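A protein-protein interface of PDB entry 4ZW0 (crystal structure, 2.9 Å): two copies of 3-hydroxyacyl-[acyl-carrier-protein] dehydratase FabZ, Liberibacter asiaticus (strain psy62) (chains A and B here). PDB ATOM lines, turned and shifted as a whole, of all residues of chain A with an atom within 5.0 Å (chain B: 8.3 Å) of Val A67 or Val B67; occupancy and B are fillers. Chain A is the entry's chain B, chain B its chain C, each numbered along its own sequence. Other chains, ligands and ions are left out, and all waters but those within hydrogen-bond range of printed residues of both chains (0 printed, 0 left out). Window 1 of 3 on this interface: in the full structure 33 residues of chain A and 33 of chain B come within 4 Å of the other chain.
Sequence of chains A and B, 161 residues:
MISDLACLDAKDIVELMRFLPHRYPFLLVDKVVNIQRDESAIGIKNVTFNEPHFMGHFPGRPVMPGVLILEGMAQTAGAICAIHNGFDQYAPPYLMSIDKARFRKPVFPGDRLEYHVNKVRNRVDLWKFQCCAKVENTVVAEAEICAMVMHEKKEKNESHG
O of Phe B26 sits at hydrogen-bond distance from NE2 of Gln B75 (3.0 Å). The side-chain amide nitrogen of Gln B75 is in hydrogen-bond range of the side-chain carboxylate of Glu B71, at 2.8 Å.
Among the printed residues, merely in contact across the chains: Phe A26 with His B57, Phe A26 with Pro B65, Phe A26 with Leu B68, Pro A65 with Phe B26, Val A67 with Phe B26, Val A67 with Val B67, Val A67 with Glu B71, Leu A68 with Phe B26, Leu A70 with Ile B98, Glu A71 with Val B67, Leu A95 with Phe B103, Ile A98 with Leu B70 and Phe A103 with Leu B95.
Val A67 touches just these residues of chain B: Phe B26 (3.9 Å), Val B67 (3.6 Å) and Glu B71 (3.7 Å). Val B67 touches just these residues of chain A: Val A67 (3.6 Å) and Glu A71 (3.6 Å). Of the printed residues of chain B, Glu A71 touches Val B67. Of the printed residues of chain B, Pro A65 touches Phe B26 (3.8 Å). Gln B75 touches none of the printed residues of chain A. Gly B72 touches none of the printed residues of chain A. The nearest residue of chain B that does not touch Val A67 is Leu B95 (4.3 Å). The nearest printed residue of chain B that does not touch Glu A71 is His B57 (4.5 Å).
Along chain A the printed residues that touch a printed residue of chain B span positions 26 to 103. Among the printed residues, no Asp or Glu carboxylate lies within 4 Å of a Lys or Arg side-chain nitrogen of the other chain.
Phe A26 touches Pro B65, and with the chains exchanged Pro A65 touches Phe B26. Val A67 touches Glu B71, and with the chains exchanged Glu A71 touches Val B67. Leu A70 touches Ile B98, and with the chains exchanged Ile A98 touches Leu B70. Leu A95 touches Phe B103, and with the chains exchanged Phe A103 touches Leu B95. 11 positions are printed for both chains.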
ATOM      1  N   PHE A  26       8.256  23.723  -5.919  1.00  0.00           N
ATOM      2  CA  PHE A  26       9.624  23.268  -6.087  1.00  0.00           C
ATOM      3  C   PHE A  26       9.816  21.843  -5.623  1.00  0.00           C
ATOM      4  O   PHE A  26      10.938  21.412  -5.319  1.00  0.00           O
ATOM      5  CB  PHE A  26      10.582  24.190  -5.358  1.00  0.00           C
ATOM      6  CG  PHE A  26      11.755  24.548  -6.173  1.00  0.00           C
ATOM      7  CD1 PHE A  26      11.679  25.592  -7.081  1.00  0.00           C
ATOM      8  CD2 PHE A  26      12.935  23.808  -6.076  1.00  0.00           C
ATOM      9  CE1 PHE A  26      12.793  25.901  -7.886  1.00  0.00           C
ATOM     10  CE2 PHE A  26      14.034  24.109  -6.861  1.00  0.00           C
ATOM     11  CZ  PHE A  26      13.973  25.154  -7.778  1.00  0.00           C
ATOM     12  N   PRO A  65      12.711  23.248 -18.486  1.00  0.00           N
ATOM     13  CA  PRO A  65      14.023  23.795 -18.156  1.00  0.00           C
ATOM     14  C   PRO A  65      14.951  22.704 -17.638  1.00  0.00           C
ATOM     15  O   PRO A  65      14.624  22.060 -16.646  1.00  0.00           O
ATOM     16  CB  PRO A  65      13.712  24.736 -16.978  1.00  0.00           C
ATOM     17  CG  PRO A  65      12.246  24.996 -17.052  1.00  0.00           C
ATOM     18  CD  PRO A  65      11.660  23.765 -17.570  1.00  0.00           C
ATOM     19  N   GLY A  66      16.112  22.549 -18.245  1.00  0.00           N
ATOM     20  CA  GLY A  66      17.063  21.551 -17.835  1.00  0.00           C
ATOM     21  C   GLY A  66      17.434  21.609 -16.383  1.00  0.00           C
ATOM     22  O   GLY A  66      17.568  20.566 -15.733  1.00  0.00           O
ATOM     23  N   VAL A  67      17.600  22.812 -15.846  1.00  0.00           N
ATOM     24  CA  VAL A  67      17.908  22.933 -14.413  1.00  0.00           C
ATOM     25  C   VAL A  67      16.862  22.281 -13.498  1.00  0.00           C
ATOM     26  O   VAL A  67      17.188  21.817 -12.422  1.00  0.00           O
ATOM     27  CB  VAL A  67      18.166  24.390 -13.991  1.00  0.00           C
ATOM     28  CG1 VAL A  67      19.422  24.934 -14.689  1.00  0.00           C
ATOM     29  CG2 VAL A  67      16.892  25.279 -14.247  1.00  0.00           C
ATOM     30  N   LEU A  68      15.604  22.236 -13.918  1.00  0.00           N
ATOM     31  CA  LEU A  68      14.586  21.561 -13.101  1.00  0.00           C
ATOM     32  C   LEU A  68      14.617  20.041 -13.323  1.00  0.00           C
ATOM     33  O   LEU A  68      14.174  19.270 -12.491  1.00  0.00           O
ATOM     34  CB  LEU A  68      13.190  22.101 -13.404  1.00  0.00           C
ATOM     35  CG  LEU A  68      13.014  23.604 -13.347  1.00  0.00           C
ATOM     36  CD1 LEU A  68      11.563  23.968 -13.578  1.00  0.00           C
ATOM     37  CD2 LEU A  68      13.461  24.051 -12.030  1.00  0.00           C
ATOM     38  N   ILE A  69      15.126  19.611 -14.455  1.00  0.00           N
ATOM     39  CA  ILE A  69      15.498  18.228 -14.567  1.00  0.00           C
ATOM     40  C   ILE A  69      16.597  17.835 -13.581  1.00  0.00           C
ATOM     41  O   ILE A  69      16.452  16.850 -12.857  1.00  0.00           O
ATOM     42  CB  ILE A  69      15.921  17.922 -15.977  1.00  0.00           C
ATOM     43  CG1 ILE A  69      14.773  18.360 -16.910  1.00  0.00           C
ATOM     44  CG2 ILE A  69      16.270  16.464 -16.093  1.00  0.00           C
ATOM     45  CD1 ILE A  69      14.938  18.013 -18.319  1.00  0.00           C
ATOM     46  N   LEU A  70      17.676  18.615 -13.547  1.00  0.00           N
ATOM     47  CA  LEU A  70      18.716  18.462 -12.525  1.00  0.00           C
ATOM     48  C   LEU A  70      18.093  18.440 -11.150  1.00  0.00           C
ATOM     49  O   LEU A  70      18.373  17.560 -10.354  1.00  0.00           O
ATOM     50  CB  LEU A  70      19.705  19.616 -12.564  1.00  0.00           C
ATOM     51  CG  LEU A  70      20.542  19.680 -13.825  1.00  0.00           C
ATOM     52  CD1 LEU A  70      21.546  20.804 -13.730  1.00  0.00           C
ATOM     53  CD2 LEU A  70      21.211  18.334 -14.013  1.00  0.00           C
ATOM     54  N   GLU A  71      17.239  19.403 -10.859  1.00  0.00           N
ATOM     55  CA  GLU A  71      16.662  19.479  -9.541  1.00  0.00           C
ATOM     56  C   GLU A  71      15.810  18.238  -9.233  1.00  0.00           C
ATOM     57  O   GLU A  71      15.832  17.745  -8.110  1.00  0.00           O
ATOM     58  CB  GLU A  71      15.885  20.787  -9.382  1.00  0.00           C
ATOM     59  CG  GLU A  71      15.172  20.914  -8.047  1.00  0.00           C
ATOM     60  CD  GLU A  71      16.110  21.274  -6.864  1.00  0.00           C
ATOM     61  OE1 GLU A  71      17.212  21.862  -7.129  1.00  0.00           O
ATOM     62  OE2 GLU A  71      15.733  20.995  -5.669  1.00  0.00           O
ATOM     63  N   LEU A  95      22.579  21.602  -1.932  1.00  0.00           N
ATOM     64  CA  LEU A  95      23.286  21.199  -3.142  1.00  0.00           C
ATOM     65  C   LEU A  95      24.673  21.830  -3.236  1.00  0.00           C
ATOM     66  O   LEU A  95      24.833  23.068  -3.172  1.00  0.00           O
ATOM     67  CB  LEU A  95      22.484  21.632  -4.339  1.00  0.00           C
ATOM     68  CG  LEU A  95      23.044  21.122  -5.646  1.00  0.00           C
ATOM     69  CD1 LEU A  95      22.826  19.618  -5.647  1.00  0.00           C
ATOM     70  CD2 LEU A  95      22.346  21.845  -6.809  1.00  0.00           C
ATOM     71  N   ILE A  98      27.447  20.115  -9.146  1.00  0.00           N
ATOM     72  CA  ILE A  98      26.896  19.397 -10.283  1.00  0.00           C
ATOM     73  C   ILE A  98      28.004  19.295 -11.311  1.00  0.00           C
ATOM     74  O   ILE A  98      28.644  20.297 -11.637  1.00  0.00           O
ATOM     75  CB  ILE A  98      25.691  20.105 -10.892  1.00  0.00           C
ATOM     76  CG1 ILE A  98      24.634  20.367  -9.812  1.00  0.00           C
ATOM     77  CG2 ILE A  98      25.099  19.264 -12.013  1.00  0.00           C
ATOM     78  CD1 ILE A  98      23.447  21.155 -10.286  1.00  0.00           C
ATOM     79  N   PHE A 103      22.627  17.607 -21.495  1.00  0.00           N
ATOM     80  CA  PHE A 103      21.216  17.584 -21.899  1.00  0.00           C
ATOM     81  C   PHE A 103      21.122  17.213 -23.365  1.00  0.00           C
ATOM     82  O   PHE A 103      21.647  17.915 -24.217  1.00  0.00           O
ATOM     83  CB  PHE A 103      20.544  18.934 -21.635  1.00  0.00           C
ATOM     84  CG  PHE A 103      20.610  19.373 -20.192  1.00  0.00           C
ATOM     85  CD1 PHE A 103      19.819  18.763 -19.210  1.00  0.00           C
ATOM     86  CD2 PHE A 103      21.474  20.384 -19.809  1.00  0.00           C
ATOM     87  CE1 PHE A 103      19.898  19.152 -17.893  1.00  0.00           C
ATOM     88  CE2 PHE A 103      21.566  20.777 -18.490  1.00  0.00           C
ATOM     89  CZ  PHE A 103      20.771  20.160 -17.523  1.00  0.00           C
ATOM     90  N   PHE B  26      10.414  32.766 -14.695  1.00  0.00           N
ATOM     91  CA  PHE B  26      11.676  32.150 -15.038  1.00  0.00           C
ATOM     92  C   PHE B  26      12.673  33.113 -15.665  1.00  0.00           C
ATOM     93  O   PHE B  26      13.601  32.705 -16.358  1.00  0.00           O
ATOM     94  CB  PHE B  26      11.441  30.914 -15.907  1.00  0.00           C
ATOM     95  CG  PHE B  26      12.230  29.745 -15.457  1.00  0.00           C
ATOM     96  CD1 PHE B  26      11.738  28.902 -14.478  1.00  0.00           C
ATOM     97  CD2 PHE B  26      13.513  29.517 -15.955  1.00  0.00           C
ATOM     98  CE1 PHE B  26      12.522  27.813 -14.005  1.00  0.00           C
ATOM     99  CE2 PHE B  26      14.290  28.441 -15.504  1.00  0.00           C
ATOM    100  CZ  PHE B  26      13.805  27.595 -14.520  1.00  0.00           C
ATOM    101  N   LEU B  28      15.447  35.338 -14.565  1.00  0.00           N
ATOM    102  CA  LEU B  28      16.170  35.274 -13.298  1.00  0.00           C
ATOM    103  C   LEU B  28      17.381  36.175 -13.225  1.00  0.00           C
ATOM    104  O   LEU B  28      18.275  35.959 -12.419  1.00  0.00           O
ATOM    105  CB  LEU B  28      16.516  33.821 -12.929  1.00  0.00           C
ATOM    106  CG  LEU B  28      15.272  32.906 -12.825  1.00  0.00           C
ATOM    107  CD1 LEU B  28      15.613  31.478 -12.459  1.00  0.00           C
ATOM    108  CD2 LEU B  28      14.254  33.472 -11.837  1.00  0.00           C
ATOM    109  N   HIS B  57      10.768  26.313  -0.962  1.00  0.00           N
ATOM    110  CA  HIS B  57      12.200  26.059  -0.882  1.00  0.00           C
ATOM    111  C   HIS B  57      12.942  27.055   0.028  1.00  0.00           C
ATOM    112  O   HIS B  57      13.767  27.859  -0.438  1.00  0.00           O
ATOM    113  CB  HIS B  57      12.802  26.035  -2.287  1.00  0.00           C
ATOM    114  CG  HIS B  57      14.197  25.480  -2.362  1.00  0.00           C
ATOM    115  ND1 HIS B  57      15.306  26.165  -1.905  1.00  0.00           N
ATOM    116  CD2 HIS B  57      14.673  24.317  -2.879  1.00  0.00           C
ATOM    117  CE1 HIS B  57      16.393  25.446  -2.123  1.00  0.00           C
ATOM    118  NE2 HIS B  57      16.035  24.317  -2.711  1.00  0.00           N
ATOM    119  N   MET B  64      17.765  30.275  -1.513  1.00  0.00           N
ATOM    120  CA  MET B  64      17.824  30.260  -2.997  1.00  0.00           C
ATOM    121  C   MET B  64      18.360  28.954  -3.542  1.00  0.00           C
ATOM    122  O   MET B  64      19.471  28.527  -3.156  1.00  0.00           O
ATOM    123  CB  MET B  64      18.746  31.357  -3.494  1.00  0.00           C
ATOM    124  CG  MET B  64      18.975  31.344  -4.958  1.00  0.00           C
ATOM    125  SD  MET B  64      17.941  32.579  -5.755  1.00  0.00           S
ATOM    126  CE  MET B  64      18.735  32.694  -7.342  1.00  0.00           C
ATOM    127  N   PRO B  65      17.568  28.307  -4.423  1.00  0.00           N
ATOM    128  CA  PRO B  65      17.921  27.010  -5.016  1.00  0.00           C
ATOM    129  C   PRO B  65      19.116  27.202  -5.940  1.00  0.00           C
ATOM    130  O   PRO B  65      19.035  28.082  -6.818  1.00  0.00           O
ATOM    131  CB  PRO B  65      16.675  26.644  -5.839  1.00  0.00           C
ATOM    132  CG  PRO B  65      15.583  27.421  -5.228  1.00  0.00           C
ATOM    133  CD  PRO B  65      16.217  28.732  -4.816  1.00  0.00           C
ATOM    134  N   GLY B  66      20.177  26.406  -5.751  1.00  0.00           N
ATOM    135  CA  GLY B  66      21.388  26.507  -6.553  1.00  0.00           C
ATOM    136  C   GLY B  66      21.112  26.478  -8.044  1.00  0.00           C
ATOM    137  O   GLY B  66      21.631  27.331  -8.802  1.00  0.00           O
ATOM    138  N   VAL B  67      20.267  25.528  -8.461  1.00  0.00           N
ATOM    139  CA  VAL B  67      19.881  25.450  -9.864  1.00  0.00           C
ATOM    140  C   VAL B  67      19.357  26.753 -10.480  1.00  0.00           C
ATOM    141  O   VAL B  67      19.536  26.978 -11.707  1.00  0.00           O
ATOM    142  CB  VAL B  67      18.897  24.333 -10.168  1.00  0.00           C
ATOM    143  CG1 VAL B  67      19.520  22.968  -9.873  1.00  0.00           C
ATOM    144  CG2 VAL B  67      17.592  24.546  -9.431  1.00  0.00           C
ATOM    145  N   LEU B  68      18.729  27.611  -9.657  1.00  0.00           N
ATOM    146  CA  LEU B  68      18.271  28.929 -10.137  1.00  0.00           C
ATOM    147  C   LEU B  68      19.419  29.924 -10.181  1.00  0.00           C
ATOM    148  O   LEU B  68      19.409  30.895 -10.939  1.00  0.00           O
ATOM    149  CB  LEU B  68      17.169  29.477  -9.261  1.00  0.00           C
ATOM    150  CG  LEU B  68      15.947  28.568  -9.186  1.00  0.00           C
ATOM    151  CD1 LEU B  68      14.826  29.265  -8.435  1.00  0.00           C
ATOM    152  CD2 LEU B  68      15.493  28.121 -10.555  1.00  0.00           C
ATOM    153  N   ILE B  69      20.425  29.694  -9.358  1.00  0.00           N
ATOM    154  CA  ILE B  69      21.613  30.481  -9.537  1.00  0.00           C
ATOM    155  C   ILE B  69      22.243  30.123 -10.897  1.00  0.00           C
ATOM    156  O   ILE B  69      22.615  31.021 -11.696  1.00  0.00           O
ATOM    157  CB  ILE B  69      22.550  30.248  -8.384  1.00  0.00           C
ATOM    158  CG1 ILE B  69      21.781  30.582  -7.108  1.00  0.00           C
ATOM    159  CG2 ILE B  69      23.806  31.084  -8.546  1.00  0.00           C
ATOM    160  CD1 ILE B  69      22.600  30.539  -5.874  1.00  0.00           C
ATOM    161  N   LEU B  70      22.336  28.816 -11.175  1.00  0.00           N
ATOM    162  CA  LEU B  70      22.922  28.352 -12.450  1.00  0.00           C
ATOM    163  C   LEU B  70      22.182  29.009 -13.561  1.00  0.00           C
ATOM    164  O   LEU B  70      22.786  29.589 -14.453  1.00  0.00           O
ATOM    165  CB  LEU B  70      22.798  26.837 -12.617  1.00  0.00           C
ATOM    166  CG  LEU B  70      23.720  26.038 -11.705  1.00  0.00           C
ATOM    167  CD1 LEU B  70      23.578  24.569 -12.000  1.00  0.00           C
ATOM    168  CD2 LEU B  70      25.134  26.531 -11.896  1.00  0.00           C
ATOM    169  N   GLU B  71      20.855  28.931 -13.469  1.00  0.00           N
ATOM    170  CA  GLU B  71      19.977  29.523 -14.469  1.00  0.00           C
ATOM    171  C   GLU B  71      20.167  31.043 -14.659  1.00  0.00           C
ATOM    172  O   GLU B  71      20.172  31.526 -15.788  1.00  0.00           O
ATOM    173  CB  GLU B  71      18.517  29.176 -14.172  1.00  0.00           C
ATOM    174  CG  GLU B  71      17.548  29.745 -15.209  1.00  0.00           C
ATOM    175  CD  GLU B  71      17.632  29.057 -16.596  1.00  0.00           C
ATOM    176  OE1 GLU B  71      17.993  27.845 -16.671  1.00  0.00           O
ATOM    177  OE2 GLU B  71      17.321  29.722 -17.621  1.00  0.00           O
ATOM    178  N   GLY B  72      20.357  31.770 -13.555  1.00  0.00           N
ATOM    179  CA  GLY B  72      20.727  33.183 -13.578  1.00  0.00           C
ATOM    180  C   GLY B  72      21.975  33.405 -14.404  1.00  0.00           C
ATOM    181  O   GLY B  72      21.941  34.112 -15.420  1.00  0.00           O
ATOM    182  N   MET B  73      23.070  32.774 -13.992  1.00  0.00           N
ATOM    183  CA  MET B  73      24.296  32.781 -14.785  1.00  0.00           C
ATOM    184  C   MET B  73      24.099  32.534 -16.301  1.00  0.00           C
ATOM    185  O   MET B  73      24.600  33.290 -17.158  1.00  0.00           O
ATOM    186  CB  MET B  73      25.248  31.731 -14.229  1.00  0.00           C
ATOM    187  CG  MET B  73      25.761  31.970 -12.815  1.00  0.00           C
ATOM    188  SD  MET B  73      26.695  30.483 -12.397  1.00  0.00           S
ATOM    189  CE  MET B  73      27.083  30.731 -10.668  1.00  0.00           C
ATOM    190  N   ALA B  74      23.373  31.469 -16.613  1.00  0.00           N
ATOM    191  CA  ALA B  74      23.141  31.077 -17.992  1.00  0.00           C
ATOM    192  C   ALA B  74      22.375  32.155 -18.728  1.00  0.00           C
ATOM    193  O   ALA B  74      22.603  32.404 -19.920  1.00  0.00           O
ATOM    194  CB  ALA B  74      22.395  29.750 -18.058  1.00  0.00           C
ATOM    195  N   GLN B  75      21.479  32.822 -18.019  1.00  0.00           N
ATOM    196  CA  GLN B  75      20.696  33.868 -18.657  1.00  0.00           C
ATOM    197  C   GLN B  75      21.515  35.094 -18.926  1.00  0.00           C
ATOM    198  O   GLN B  75      21.299  35.756 -19.922  1.00  0.00           O
ATOM    199  CB  GLN B  75      19.482  34.236 -17.822  1.00  0.00           C
ATOM    200  CG  GLN B  75      18.303  33.388 -18.171  1.00  0.00           C
ATOM    201  CD  GLN B  75      17.205  33.470 -17.168  1.00  0.00           C
ATOM    202  OE1 GLN B  75      16.975  34.506 -16.592  1.00  0.00           O
ATOM    203  NE2 GLN B  75      16.511  32.368 -16.950  1.00  0.00           N
ATOM    204  N   LEU B  95      19.927  24.936 -23.232  1.00  0.00           N
ATOM    205  CA  LEU B  95      21.046  24.566 -22.381  1.00  0.00           C
ATOM    206  C   LEU B  95      21.575  23.156 -22.669  1.00  0.00           C
ATOM    207  O   LEU B  95      20.825  22.179 -22.607  1.00  0.00           O
ATOM    208  CB  LEU B  95      20.612  24.664 -20.924  1.00  0.00           C
ATOM    209  CG  LEU B  95      21.737  24.441 -19.942  1.00  0.00           C
ATOM    210  CD1 LEU B  95      22.711  25.569 -20.065  1.00  0.00           C
ATOM    211  CD2 LEU B  95      21.171  24.352 -18.588  1.00  0.00           C
ATOM    212  N   ILE B  98      26.452  21.661 -18.229  1.00  0.00           N
ATOM    213  CA  ILE B  98      26.955  22.374 -17.071  1.00  0.00           C
ATOM    214  C   ILE B  98      28.060  21.536 -16.485  1.00  0.00           C
ATOM    215  O   ILE B  98      27.866  20.355 -16.216  1.00  0.00           O
ATOM    216  CB  ILE B  98      25.831  22.629 -16.017  1.00  0.00           C
ATOM    217  CG1 ILE B  98      24.629  23.320 -16.654  1.00  0.00           C
ATOM    218  CG2 ILE B  98      26.299  23.515 -14.874  1.00  0.00           C
ATOM    219  CD1 ILE B  98      23.500  23.435 -15.695  1.00  0.00           C
ATOM    220  N   PHE B 103      28.795  24.994  -5.422  1.00  0.00           N
ATOM    221  CA  PHE B 103      28.073  25.916  -4.545  1.00  0.00           C
ATOM    222  C   PHE B 103      28.746  26.004  -3.166  1.00  0.00           C
ATOM    223  O   PHE B 103      28.807  25.011  -2.407  1.00  0.00           O
ATOM    224  CB  PHE B 103      26.602  25.464  -4.407  1.00  0.00           C
ATOM    225  CG  PHE B 103      25.887  25.312  -5.736  1.00  0.00           C
ATOM    226  CD1 PHE B 103      25.565  26.428  -6.516  1.00  0.00           C
ATOM    227  CD2 PHE B 103      25.551  24.061  -6.213  1.00  0.00           C
ATOM    228  CE1 PHE B 103      24.916  26.284  -7.740  1.00  0.00           C
ATOM    229  CE2 PHE B 103      24.911  23.916  -7.438  1.00  0.00           C
ATOM    230  CZ  PHE B 103      24.591  25.028  -8.199  1.00  0.00           C
ATOM    231  N   TYR B 115      26.455  38.014 -11.123  1.00  0.00           N
ATOM    232  CA  TYR B 115      26.921  36.905 -11.940  1.00  0.00           C
ATOM    233  C   TYR B 115      28.003  37.408 -12.890  1.00  0.00           C
ATOM    234  O   TYR B 115      27.711  38.060 -13.905  1.00  0.00           O
ATOM    235  CB  TYR B 115      25.746  36.333 -12.756  1.00  0.00           C
ATOM    236  CG  TYR B 115      24.553  35.795 -11.959  1.00  0.00           C
ATOM    237  CD1 TYR B 115      24.722  34.880 -10.907  1.00  0.00           C
ATOM    238  CD2 TYR B 115      23.253  36.199 -12.279  1.00  0.00           C
ATOM    239  CE1 TYR B 115      23.613  34.369 -10.204  1.00  0.00           C
ATOM    240  CE2 TYR B 115      22.130  35.709 -11.577  1.00  0.00           C
ATOM    241  CZ  TYR B 115      22.309  34.785 -10.542  1.00  0.00           C
ATOM    242  OH  TYR B 115      21.198  34.276  -9.873  1.00  0.00           O
ATOM    243  N   ALA B 141      28.971  30.900  -5.723  1.00  0.00           N
ATOM    244  CA  ALA B 141      28.932  29.726  -6.619  1.00  0.00           C
ATOM    245  C   ALA B 141      29.795  29.891  -7.857  1.00  0.00           C
ATOM    246  O   ALA B 141      30.293  30.977  -8.155  1.00  0.00           O
ATOM    247  CB  ALA B 141      27.466  29.328  -7.019  1.00  0.00           C
ATOM    248  N   ILE B 145      29.182  26.871 -18.148  1.00  0.00           N
ATOM    249  CA  ILE B 145      27.869  26.619 -18.730  1.00  0.00           C
ATOM    250  C   ILE B 145      27.944  26.740 -20.221  1.00  0.00           C
ATOM    251  O   ILE B 145      28.368  27.767 -20.740  1.00  0.00           O
ATOM    252  CB  ILE B 145      26.797  27.676 -18.338  1.00  0.00           C
ATOM    253  CG1 ILE B 145      26.895  28.145 -16.877  1.00  0.00           C
ATOM    254  CG2 ILE B 145      25.426  27.158 -18.639  1.00  0.00           C
ATOM    255  CD1 ILE B 145      26.353  27.203 -15.905  1.00  0.00           C
